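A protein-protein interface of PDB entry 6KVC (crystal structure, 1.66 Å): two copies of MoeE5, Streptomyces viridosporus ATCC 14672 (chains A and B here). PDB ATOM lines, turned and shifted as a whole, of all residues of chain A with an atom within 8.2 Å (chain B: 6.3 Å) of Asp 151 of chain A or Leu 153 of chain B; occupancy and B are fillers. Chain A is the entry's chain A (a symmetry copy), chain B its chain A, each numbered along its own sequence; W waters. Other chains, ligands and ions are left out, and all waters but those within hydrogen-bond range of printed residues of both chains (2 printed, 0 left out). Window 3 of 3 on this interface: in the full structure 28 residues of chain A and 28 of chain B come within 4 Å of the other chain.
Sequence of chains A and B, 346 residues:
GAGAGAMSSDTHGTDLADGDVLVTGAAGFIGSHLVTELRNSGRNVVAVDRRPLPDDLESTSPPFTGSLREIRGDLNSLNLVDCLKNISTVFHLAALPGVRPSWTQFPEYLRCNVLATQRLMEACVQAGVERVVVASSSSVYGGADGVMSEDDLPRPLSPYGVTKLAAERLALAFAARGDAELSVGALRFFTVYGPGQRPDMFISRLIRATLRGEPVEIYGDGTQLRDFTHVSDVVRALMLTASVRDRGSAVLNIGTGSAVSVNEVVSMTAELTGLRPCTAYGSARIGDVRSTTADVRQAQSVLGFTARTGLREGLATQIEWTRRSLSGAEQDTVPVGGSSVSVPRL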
ATOM      1  N   TYR A 141       8.133 -16.460 -23.864  1.00  0.00           N
ATOM      2  CA  TYR A 141       8.788 -15.192 -23.515  1.00  0.00           C
ATOM      3  C   TYR A 141       9.563 -14.602 -24.669  1.00  0.00           C
ATOM      4  O   TYR A 141       9.764 -13.396 -24.694  1.00  0.00           O
ATOM      5  CB  TYR A 141       9.748 -15.394 -22.329  1.00  0.00           C
ATOM      6  CG  TYR A 141       9.010 -15.767 -21.061  1.00  0.00           C
ATOM      7  CD1 TYR A 141       8.048 -14.917 -20.526  1.00  0.00           C
ATOM      8  CD2 TYR A 141       9.213 -17.000 -20.457  1.00  0.00           C
ATOM      9  CE1 TYR A 141       7.368 -15.250 -19.359  1.00  0.00           C
ATOM     10  CE2 TYR A 141       8.520 -17.363 -19.292  1.00  0.00           C
ATOM     11  CZ  TYR A 141       7.607 -16.473 -18.751  1.00  0.00           C
ATOM     12  OH  TYR A 141       6.918 -16.801 -17.621  1.00  0.00           O
ATOM     13  N   VAL A 147      16.102 -12.525 -16.102  1.00  0.00           N
ATOM     14  CA  VAL A 147      15.095 -13.410 -15.539  1.00  0.00           C
ATOM     15  C   VAL A 147      13.775 -13.205 -16.281  1.00  0.00           C
ATOM     16  O   VAL A 147      13.355 -12.068 -16.527  1.00  0.00           O
ATOM     17  CB  VAL A 147      14.970 -13.149 -14.034  1.00  0.00           C
ATOM     18  CG1 VAL A 147      13.810 -13.816 -13.528  1.00  0.00           C
ATOM     19  CG2 VAL A 147      16.204 -13.678 -13.312  1.00  0.00           C
ATOM     20  N   MET A 148      13.131 -14.307 -16.649  1.00  0.00           N
ATOM     21  CA  MET A 148      11.826 -14.309 -17.333  1.00  0.00           C
ATOM     22  C   MET A 148      10.754 -14.616 -16.298  1.00  0.00           C
ATOM     23  O   MET A 148      10.725 -15.712 -15.722  1.00  0.00           O
ATOM     24  CB  MET A 148      11.818 -15.357 -18.444  1.00  0.00           C
ATOM     25  CG  MET A 148      12.747 -15.015 -19.591  1.00  0.00           C
ATOM     26  SD  MET A 148      13.095 -16.495 -20.590  1.00  0.00           S
ATOM     27  CE  MET A 148      13.741 -15.750 -22.094  1.00  0.00           C
ATOM     28  N   SER A 149       9.869 -13.652 -16.053  1.00  0.00           N
ATOM     29  CA  SER A 149       8.877 -13.758 -15.001  1.00  0.00           C
ATOM     30  C   SER A 149       7.494 -13.925 -15.607  1.00  0.00           C
ATOM     31  O   SER A 149       7.237 -13.443 -16.720  1.00  0.00           O
ATOM     32  CB  SER A 149       8.890 -12.498 -14.129  1.00  0.00           C
ATOM     33  OG  SER A 149       7.743 -12.469 -13.324  1.00  0.00           O
ATOM     34  N   GLU A 150       6.617 -14.569 -14.837  1.00  0.00           N
ATOM     35  CA  GLU A 150       5.265 -14.821 -15.321  1.00  0.00           C
ATOM     36  C   GLU A 150       4.461 -13.535 -15.450  1.00  0.00           C
ATOM     37  O   GLU A 150       3.397 -13.567 -16.074  1.00  0.00           O
ATOM     38  CB  GLU A 150       4.526 -15.805 -14.409  1.00  0.00           C
ATOM     39  CG  GLU A 150       5.200 -17.206 -14.300  1.00  0.00           C
ATOM     40  CD  GLU A 150       6.193 -17.301 -13.131  1.00  0.00           C
ATOM     41  OE1 GLU A 150       6.461 -18.429 -12.688  1.00  0.00           O
ATOM     42  OE2 GLU A 150       6.717 -16.257 -12.674  1.00  0.00           O
ATOM     43  N   ASP A 151       4.937 -12.411 -14.905  1.00  0.00           N
ATOM     44  CA  ASP A 151       4.230 -11.165 -15.214  1.00  0.00           C
ATOM     45  C   ASP A 151       4.769 -10.444 -16.449  1.00  0.00           C
ATOM     46  O   ASP A 151       4.316  -9.325 -16.737  1.00  0.00           O
ATOM     47  CB  ASP A 151       4.187 -10.227 -14.010  1.00  0.00           C
ATOM     48  CG  ASP A 151       5.511  -9.979 -13.416  1.00  0.00           C
ATOM     49  OD1 ASP A 151       6.542 -10.377 -13.983  1.00  0.00           O
ATOM     50  OD2 ASP A 151       5.520  -9.353 -12.336  1.00  0.00           O
ATOM     51  N   ASP A 152       5.726 -11.020 -17.200  1.00  0.00           N
ATOM     52  CA  ASP A 152       6.251 -10.353 -18.385  1.00  0.00           C
ATOM     53  C   ASP A 152       5.335 -10.611 -19.563  1.00  0.00           C
ATOM     54  O   ASP A 152       4.768 -11.689 -19.676  1.00  0.00           O
ATOM     55  CB  ASP A 152       7.647 -10.882 -18.721  1.00  0.00           C
ATOM     56  CG  ASP A 152       8.672 -10.526 -17.670  1.00  0.00           C
ATOM     57  OD1 ASP A 152       8.471  -9.544 -16.951  1.00  0.00           O
ATOM     58  OD2 ASP A 152       9.693 -11.216 -17.591  1.00  0.00           O
ATOM     59  N   LEU A 153       5.156  -9.607 -20.423  1.00  0.00           N
ATOM     60  CA  LEU A 153       4.289  -9.843 -21.590  1.00  0.00           C
ATOM     61  C   LEU A 153       4.883 -10.916 -22.509  1.00  0.00           C
ATOM     62  O   LEU A 153       6.044 -10.784 -22.942  1.00  0.00           O
ATOM     63  CB  LEU A 153       4.125  -8.555 -22.395  1.00  0.00           C
ATOM     64  CG  LEU A 153       3.339  -7.466 -21.667  1.00  0.00           C
ATOM     65  CD1 LEU A 153       3.394  -6.195 -22.518  1.00  0.00           C
ATOM     66  CD2 LEU A 153       1.889  -7.884 -21.528  1.00  0.00           C
ATOM     67  N   PRO A 154       4.141 -11.962 -22.851  1.00  0.00           N
ATOM     68  CA  PRO A 154       4.676 -12.932 -23.849  1.00  0.00           C
ATOM     69  C   PRO A 154       4.956 -12.287 -25.201  1.00  0.00           C
ATOM     70  O   PRO A 154       4.206 -11.448 -25.697  1.00  0.00           O
ATOM     71  CB  PRO A 154       3.552 -13.981 -23.950  1.00  0.00           C
ATOM     72  CG  PRO A 154       2.930 -13.908 -22.483  1.00  0.00           C
ATOM     73  CD  PRO A 154       2.855 -12.415 -22.277  1.00  0.00           C
ATOM     74  N   ARG A 169      -3.231 -20.200 -23.401  1.00  0.00           N
ATOM     75  CA  ARG A 169      -4.382 -19.282 -23.291  1.00  0.00           C
ATOM     76  C   ARG A 169      -5.718 -19.991 -23.555  1.00  0.00           C
ATOM     77  O   ARG A 169      -6.733 -19.654 -22.927  1.00  0.00           O
ATOM     78  CB  ARG A 169      -4.217 -18.124 -24.253  1.00  0.00           C
ATOM     79  CG  ARG A 169      -2.967 -17.251 -23.970  1.00  0.00           C
ATOM     80  CD  ARG A 169      -3.044 -16.419 -22.648  1.00  0.00           C
ATOM     81  NE  ARG A 169      -2.164 -16.986 -21.607  1.00  0.00           N
ATOM     82  CZ  ARG A 169      -2.085 -16.502 -20.356  1.00  0.00           C
ATOM     83  NH1 ARG A 169      -1.249 -17.060 -19.466  1.00  0.00           N
ATOM     84  NH2 ARG A 169      -2.836 -15.460 -19.981  1.00  0.00           N
ATOM     85  N   ARG A 188       5.258 -23.451 -17.610  1.00  0.00           N
ATOM     86  CA  ARG A 188       6.185 -23.004 -18.640  1.00  0.00           C
ATOM     87  C   ARG A 188       7.529 -23.666 -18.346  1.00  0.00           C
ATOM     88  O   ARG A 188       8.298 -23.183 -17.521  1.00  0.00           O
ATOM     89  CB  ARG A 188       6.272 -21.486 -18.655  1.00  0.00           C
ATOM     90  CG  ARG A 188       5.007 -20.889 -19.231  1.00  0.00           C
ATOM     91  CD  ARG A 188       4.987 -19.376 -18.995  1.00  0.00           C
ATOM     92  NE  ARG A 188       3.751 -18.793 -19.546  1.00  0.00           N
ATOM     93  CZ  ARG A 188       3.446 -17.488 -19.497  1.00  0.00           C
ATOM     94  NH1 ARG A 188       4.262 -16.626 -18.876  1.00  0.00           N
ATOM     95  NH2 ARG A 188       2.309 -17.045 -20.076  1.00  0.00           N
ATOM     96  N   VAL A 251      -0.349 -19.991 -13.691  1.00  0.00           N
ATOM     97  CA  VAL A 251       0.635 -20.012 -14.775  1.00  0.00           C
ATOM     98  C   VAL A 251       1.994 -19.916 -14.090  1.00  0.00           C
ATOM     99  O   VAL A 251       2.289 -18.900 -13.458  1.00  0.00           O
ATOM    100  CB  VAL A 251       0.432 -18.854 -15.763  1.00  0.00           C
ATOM    101  CG1 VAL A 251       1.517 -18.779 -16.793  1.00  0.00           C
ATOM    102  CG2 VAL A 251      -0.971 -18.989 -16.500  1.00  0.00           C
ATOM    103  N   ASN A 253       6.384 -20.747 -14.119  1.00  0.00           N
ATOM    104  CA  ASN A 253       7.655 -21.220 -14.683  1.00  0.00           C
ATOM    105  C   ASN A 253       8.140 -22.455 -13.943  1.00  0.00           C
ATOM    106  O   ASN A 253       8.161 -22.464 -12.707  1.00  0.00           O
ATOM    107  CB  ASN A 253       8.742 -20.153 -14.533  1.00  0.00           C
ATOM    108  CG  ASN A 253       8.496 -18.906 -15.363  1.00  0.00           C
ATOM    109  OD1 ASN A 253       7.814 -18.904 -16.393  1.00  0.00           O
ATOM    110  ND2 ASN A 253       9.109 -17.835 -14.928  1.00  0.00           N
ATOM    111  N   ASP A 295      12.490 -17.091 -13.782  1.00  0.00           N
ATOM    112  CA  ASP A 295      12.146 -16.633 -12.433  1.00  0.00           C
ATOM    113  C   ASP A 295      11.488 -17.796 -11.720  1.00  0.00           C
ATOM    114  O   ASP A 295      10.443 -18.274 -12.167  1.00  0.00           O
ATOM    115  CB  ASP A 295      11.214 -15.425 -12.539  1.00  0.00           C
ATOM    116  CG  ASP A 295      10.945 -14.750 -11.191  1.00  0.00           C
ATOM    117  OD1 ASP A 295      11.343 -15.282 -10.154  1.00  0.00           O
ATOM    118  OD2 ASP A 295      10.354 -13.651 -11.206  1.00  0.00           O
ATOM    119  N   ARG A 297      10.412 -17.948  -8.584  1.00  0.00           N
ATOM    120  CA  ARG A 297       9.749 -17.607  -7.338  1.00  0.00           C
ATOM    121  C   ARG A 297       8.310 -18.086  -7.272  1.00  0.00           C
ATOM    122  O   ARG A 297       7.882 -18.602  -6.238  1.00  0.00           O
ATOM    123  CB  ARG A 297       9.797 -16.119  -7.124  1.00  0.00           C
ATOM    124  CG  ARG A 297      11.200 -15.664  -6.757  1.00  0.00           C
ATOM    125  CD  ARG A 297      11.243 -14.180  -6.622  1.00  0.00           C
ATOM    126  NE  ARG A 297      11.127 -13.483  -7.911  1.00  0.00           N
ATOM    127  CZ  ARG A 297      11.098 -12.168  -8.059  1.00  0.00           C
ATOM    128  NH1 ARG A 297      11.170 -11.353  -6.976  1.00  0.00           N
ATOM    129  NH2 ARG A 297      10.994 -11.656  -9.293  1.00  0.00           N
ATOM    130  N   GLN A 298       7.508 -17.858  -8.331  1.00  0.00           N
ATOM    131  CA  GLN A 298       6.080 -18.173  -8.181  1.00  0.00           C
ATOM    132  C   GLN A 298       5.840 -19.673  -8.017  1.00  0.00           C
ATOM    133  O   GLN A 298       4.947 -20.087  -7.264  1.00  0.00           O
ATOM    134  CB  GLN A 298       5.287 -17.579  -9.369  1.00  0.00           C
ATOM    135  CG  GLN A 298       5.348 -16.073  -9.371  1.00  0.00           C
ATOM    136  CD  GLN A 298       4.436 -15.388 -10.412  1.00  0.00           C
ATOM    137  OE1 GLN A 298       3.364 -15.895 -10.721  1.00  0.00           O
ATOM    138  NE2 GLN A 298       4.885 -14.246 -10.964  1.00  0.00           N
ATOM    139  N   VAL B 140      -8.239  -9.785 -27.057  1.00  0.00           N
ATOM    140  CA  VAL B 140      -7.089 -10.421 -26.415  1.00  0.00           C
ATOM    141  C   VAL B 140      -7.071 -10.159 -24.924  1.00  0.00           C
ATOM    142  O   VAL B 140      -6.432 -10.898 -24.191  1.00  0.00           O
ATOM    143  CB  VAL B 140      -5.737  -9.986 -27.046  1.00  0.00           C
ATOM    144  CG1 VAL B 140      -5.721 -10.222 -28.589  1.00  0.00           C
ATOM    145  CG2 VAL B 140      -5.393  -8.501 -26.688  1.00  0.00           C
ATOM    146  N   TYR B 141      -7.762  -9.117 -24.451  1.00  0.00           N
ATOM    147  CA  TYR B 141      -7.748  -8.791 -23.019  1.00  0.00           C
ATOM    148  C   TYR B 141      -8.652  -9.690 -22.210  1.00  0.00           C
ATOM    149  O   TYR B 141      -8.415  -9.855 -21.021  1.00  0.00           O
ATOM    150  CB  TYR B 141      -8.178  -7.330 -22.798  1.00  0.00           C
ATOM    151  CG  TYR B 141      -7.185  -6.352 -23.389  1.00  0.00           C
ATOM    152  CD1 TYR B 141      -5.862  -6.342 -22.963  1.00  0.00           C
ATOM    153  CD2 TYR B 141      -7.552  -5.508 -24.429  1.00  0.00           C
ATOM    154  CE1 TYR B 141      -4.944  -5.444 -23.499  1.00  0.00           C
ATOM    155  CE2 TYR B 141      -6.635  -4.611 -24.997  1.00  0.00           C
ATOM    156  CZ  TYR B 141      -5.336  -4.586 -24.514  1.00  0.00           C
ATOM    157  OH  TYR B 141      -4.423  -3.726 -25.050  1.00  0.00           O
ATOM    158  N   SER B 149      -5.245  -1.812 -20.958  1.00  0.00           N
ATOM    159  CA  SER B 149      -4.027  -1.168 -21.409  1.00  0.00           C
ATOM    160  C   SER B 149      -3.139  -2.176 -22.117  1.00  0.00           C
ATOM    161  O   SER B 149      -3.183  -3.376 -21.806  1.00  0.00           O
ATOM    162  CB  SER B 149      -3.263  -0.582 -20.216  1.00  0.00           C
ATOM    163  OG  SER B 149      -1.962  -0.243 -20.610  1.00  0.00           O
ATOM    164  N   GLU B 150      -2.314  -1.658 -23.026  1.00  0.00           N
ATOM    165  CA  GLU B 150      -1.433  -2.528 -23.797  1.00  0.00           C
ATOM    166  C   GLU B 150      -0.351  -3.152 -22.928  1.00  0.00           C
ATOM    167  O   GLU B 150       0.304  -4.090 -23.389  1.00  0.00           O
ATOM    168  CB  GLU B 150      -0.790  -1.771 -24.963  1.00  0.00           C
ATOM    169  CG  GLU B 150      -1.809  -1.190 -25.990  1.00  0.00           C
ATOM    170  CD  GLU B 150      -2.238   0.247 -25.657  1.00  0.00           C
ATOM    171  OE1 GLU B 150      -2.686   0.946 -26.579  1.00  0.00           O
ATOM    172  OE2 GLU B 150      -2.146   0.666 -24.478  1.00  0.00           O
ATOM    173  N   ASP B 151      -0.157  -2.683 -21.691  1.00  0.00           N
ATOM    174  CA  ASP B 151       0.759  -3.431 -20.827  1.00  0.00           C
ATOM    175  C   ASP B 151       0.070  -4.509 -19.991  1.00  0.00           C
ATOM    176  O   ASP B 151       0.734  -5.128 -19.144  1.00  0.00           O
ATOM    177  CB  ASP B 151       1.588  -2.502 -19.944  1.00  0.00           C
ATOM    178  CG  ASP B 151       0.773  -1.539 -19.184  1.00  0.00           C
ATOM    179  OD1 ASP B 151      -0.465  -1.634 -19.168  1.00  0.00           O
ATOM    180  OD2 ASP B 151       1.401  -0.651 -18.571  1.00  0.00           O
ATOM    181  N   ASP B 152      -1.238  -4.768 -20.173  1.00  0.00           N
ATOM    182  CA  ASP B 152      -1.915  -5.795 -19.390  1.00  0.00           C
ATOM    183  C   ASP B 152      -1.678  -7.152 -20.018  1.00  0.00           C
ATOM    184  O   ASP B 152      -1.612  -7.264 -21.234  1.00  0.00           O
ATOM    185  CB  ASP B 152      -3.421  -5.527 -19.346  1.00  0.00           C
ATOM    186  CG  ASP B 152      -3.766  -4.266 -18.590  1.00  0.00           C
ATOM    187  OD1 ASP B 152      -2.975  -3.846 -17.741  1.00  0.00           O
ATOM    188  OD2 ASP B 152      -4.847  -3.718 -18.828  1.00  0.00           O
ATOM    189  N   LEU B 153      -1.511  -8.183 -19.188  1.00  0.00           N
ATOM    190  CA  LEU B 153      -1.304  -9.518 -19.776  1.00  0.00           C
ATOM    191  C   LEU B 153      -2.539  -9.969 -20.563  1.00  0.00           C
ATOM    192  O   LEU B 153      -3.653  -9.989 -20.004  1.00  0.00           O
ATOM    193  CB  LEU B 153      -1.029 -10.542 -18.677  1.00  0.00           C
ATOM    194  CG  LEU B 153       0.302 -10.336 -17.957  1.00  0.00           C
ATOM    195  CD1 LEU B 153       0.366 -11.324 -16.791  1.00  0.00           C
ATOM    196  CD2 LEU B 153       1.450 -10.637 -18.900  1.00  0.00           C
ATOM    197  N   PRO B 154      -2.400 -10.358 -21.824  1.00  0.00           N
ATOM    198  CA  PRO B 154      -3.581 -10.922 -22.540  1.00  0.00           C
ATOM    199  C   PRO B 154      -4.120 -12.183 -21.878  1.00  0.00           C
ATOM    200  O   PRO B 154      -3.381 -13.048 -21.410  1.00  0.00           O
ATOM    201  CB  PRO B 154      -3.023 -11.220 -23.945  1.00  0.00           C
ATOM    202  CG  PRO B 154      -1.899 -10.097 -24.076  1.00  0.00           C
ATOM    203  CD  PRO B 154      -1.237 -10.196 -22.722  1.00  0.00           C
ATOM    204  N   ARG B 155      -5.448 -12.280 -21.842  1.00  0.00           N
ATOM    205  CA  ARG B 155      -6.130 -13.412 -21.230  1.00  0.00           C
ATOM    206  C   ARG B 155      -7.465 -13.548 -21.935  1.00  0.00           C
ATOM    207  O   ARG B 155      -8.530 -13.374 -21.332  1.00  0.00           O
ATOM    208  CB  ARG B 155      -6.306 -13.211 -19.728  1.00  0.00           C
ATOM    209  CG  ARG B 155      -6.624 -14.548 -19.012  1.00  0.00           C
ATOM    210  CD  ARG B 155      -6.701 -14.397 -17.492  1.00  0.00           C
ATOM    211  NE  ARG B 155      -7.061 -15.651 -16.821  1.00  0.00           N
ATOM    212  CZ  ARG B 155      -6.229 -16.399 -16.091  1.00  0.00           C
ATOM    213  NH1 ARG B 155      -4.939 -16.038 -15.911  1.00  0.00           N
ATOM    214  NH2 ARG B 155      -6.700 -17.516 -15.530  1.00  0.00           N
HETATM  215  O   HOH W   1      -0.563 -13.473 -21.744  1.00  0.00           O
HETATM  216  O   HOH W   2      -3.121 -14.210 -17.200  1.00  0.00           O
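Printed residues of chain B within 4 Å of Asp 151 of chain A: Leu 153 (3.8 Å). Of the printed residues of chain B, Asp 152 of chain A touches Leu 153 (3.6 Å). Pro 154 of chain A touches none of the printed residues of chain B. Arg 297 of chain A touches none of the printed residues of chain B. Printed residues of chain A within 4 Å of Glu 150 of chain B: Leu 153. Of chain A, only Arg 169 (2.9 Å) comes within 4 Å of Pro 154 of chain B. The nearest printed residue of chain B that does not touch Asp 151 of chain A is Asp 151 of chain B (6.0 Å).
Of the 16 printed residues of chain A, 5 touch a printed residue of chain B. Along chain A the printed residues that touch a printed residue of chain B span positions 150 to 169. Printed residues of chain B that touch a printed residue of chain A: Glu 150, Asp 151, Asp 152, Leu 153 and Pro 154. Hydrophobic or aromatic side chains of chain B that line the printed part of chain A: Leu 153. Among the printed residues, 8 pairs touch across the chains.
Water W1 bridges O of Pro 154 of chain B and NH2 of Arg 169 of chain A. Water W2 lies within hydrogen-bond range of NH1 of Arg 155 of chain B (2.9 Å) and NH2 of Arg 169 of chain A (3.1 Å).
OG of Ser 149 of chain B sits at hydrogen-bond distance from OD1 of Asp 151 of chain B (2.5 Å). The side-chain hydroxyl (OG) of Ser 149 of chain A lies within hydrogen-bond range of the side-chain carboxylate (OD1) of Asp 151 of chain A. The backbone NH (N) of Ser 149 of chain B lies within hydrogen-bond range of the side-chain carboxylate (OD2) of Asp 152 of chain B, 2.9 Å away. The side-chain carboxylate of Glu 150 of chain A lies within hydrogen-bond range of the side-chain amide nitrogen of Gln 298 of chain A (3.2 Å). N of Ser 149 of chain A lies within hydrogen-bond range of OD2 of Asp 152 of chain A (2.9 Å). The side-chain carboxylate of Glu 150 of chain A is in hydrogen-bond range of the backbone NH of Asn 253 of chain A (2.7 Å).
Glu 150 of chain A touches Leu 153 of chain B, and with the chains exchanged Leu 153 of chain A touches Glu 150 of chain B. Asp 151 of chain A touches Leu 153 of chain B, and with the chains exchanged Leu 153 of chain A touches Asp 151 of chain B. Asp 152 of chain A touches Leu 153 of chain B, and with the chains exchanged Leu 153 of chain A touches Asp 152 of chain B. Leu 153 of chain B touches its own counterpart, Leu 153 of chain A. Positions printed for both chains: 141, 149, 150, 151, 152, 153 and 154.
The guanidinium group of Arg 169 of chain A sits at hydrogen-bond distance from the backbone carbonyl oxygen of Pro 154 of chain B, 2.9 Å away.
Leu 153 of chain B touches Glu 150 of chain A. CD2 of Leu 153 of chain B touches O of Asp 151 of chain A (3.8 Å). O of Asp 152 of chain A touches CD2 of Leu 153 of chain B, 3.6 Å away. Leu 153 of chain A touches Glu 150 of chain B (CD1 to O, 3.8 Å). Leu 153 of chain A touches Asp 151 of chain B. Asp 152 of chain B touches Leu 153 of chain A (O to CD2, 3.6 Å). Leu 153 of chain B touches Leu 153 of chain A.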
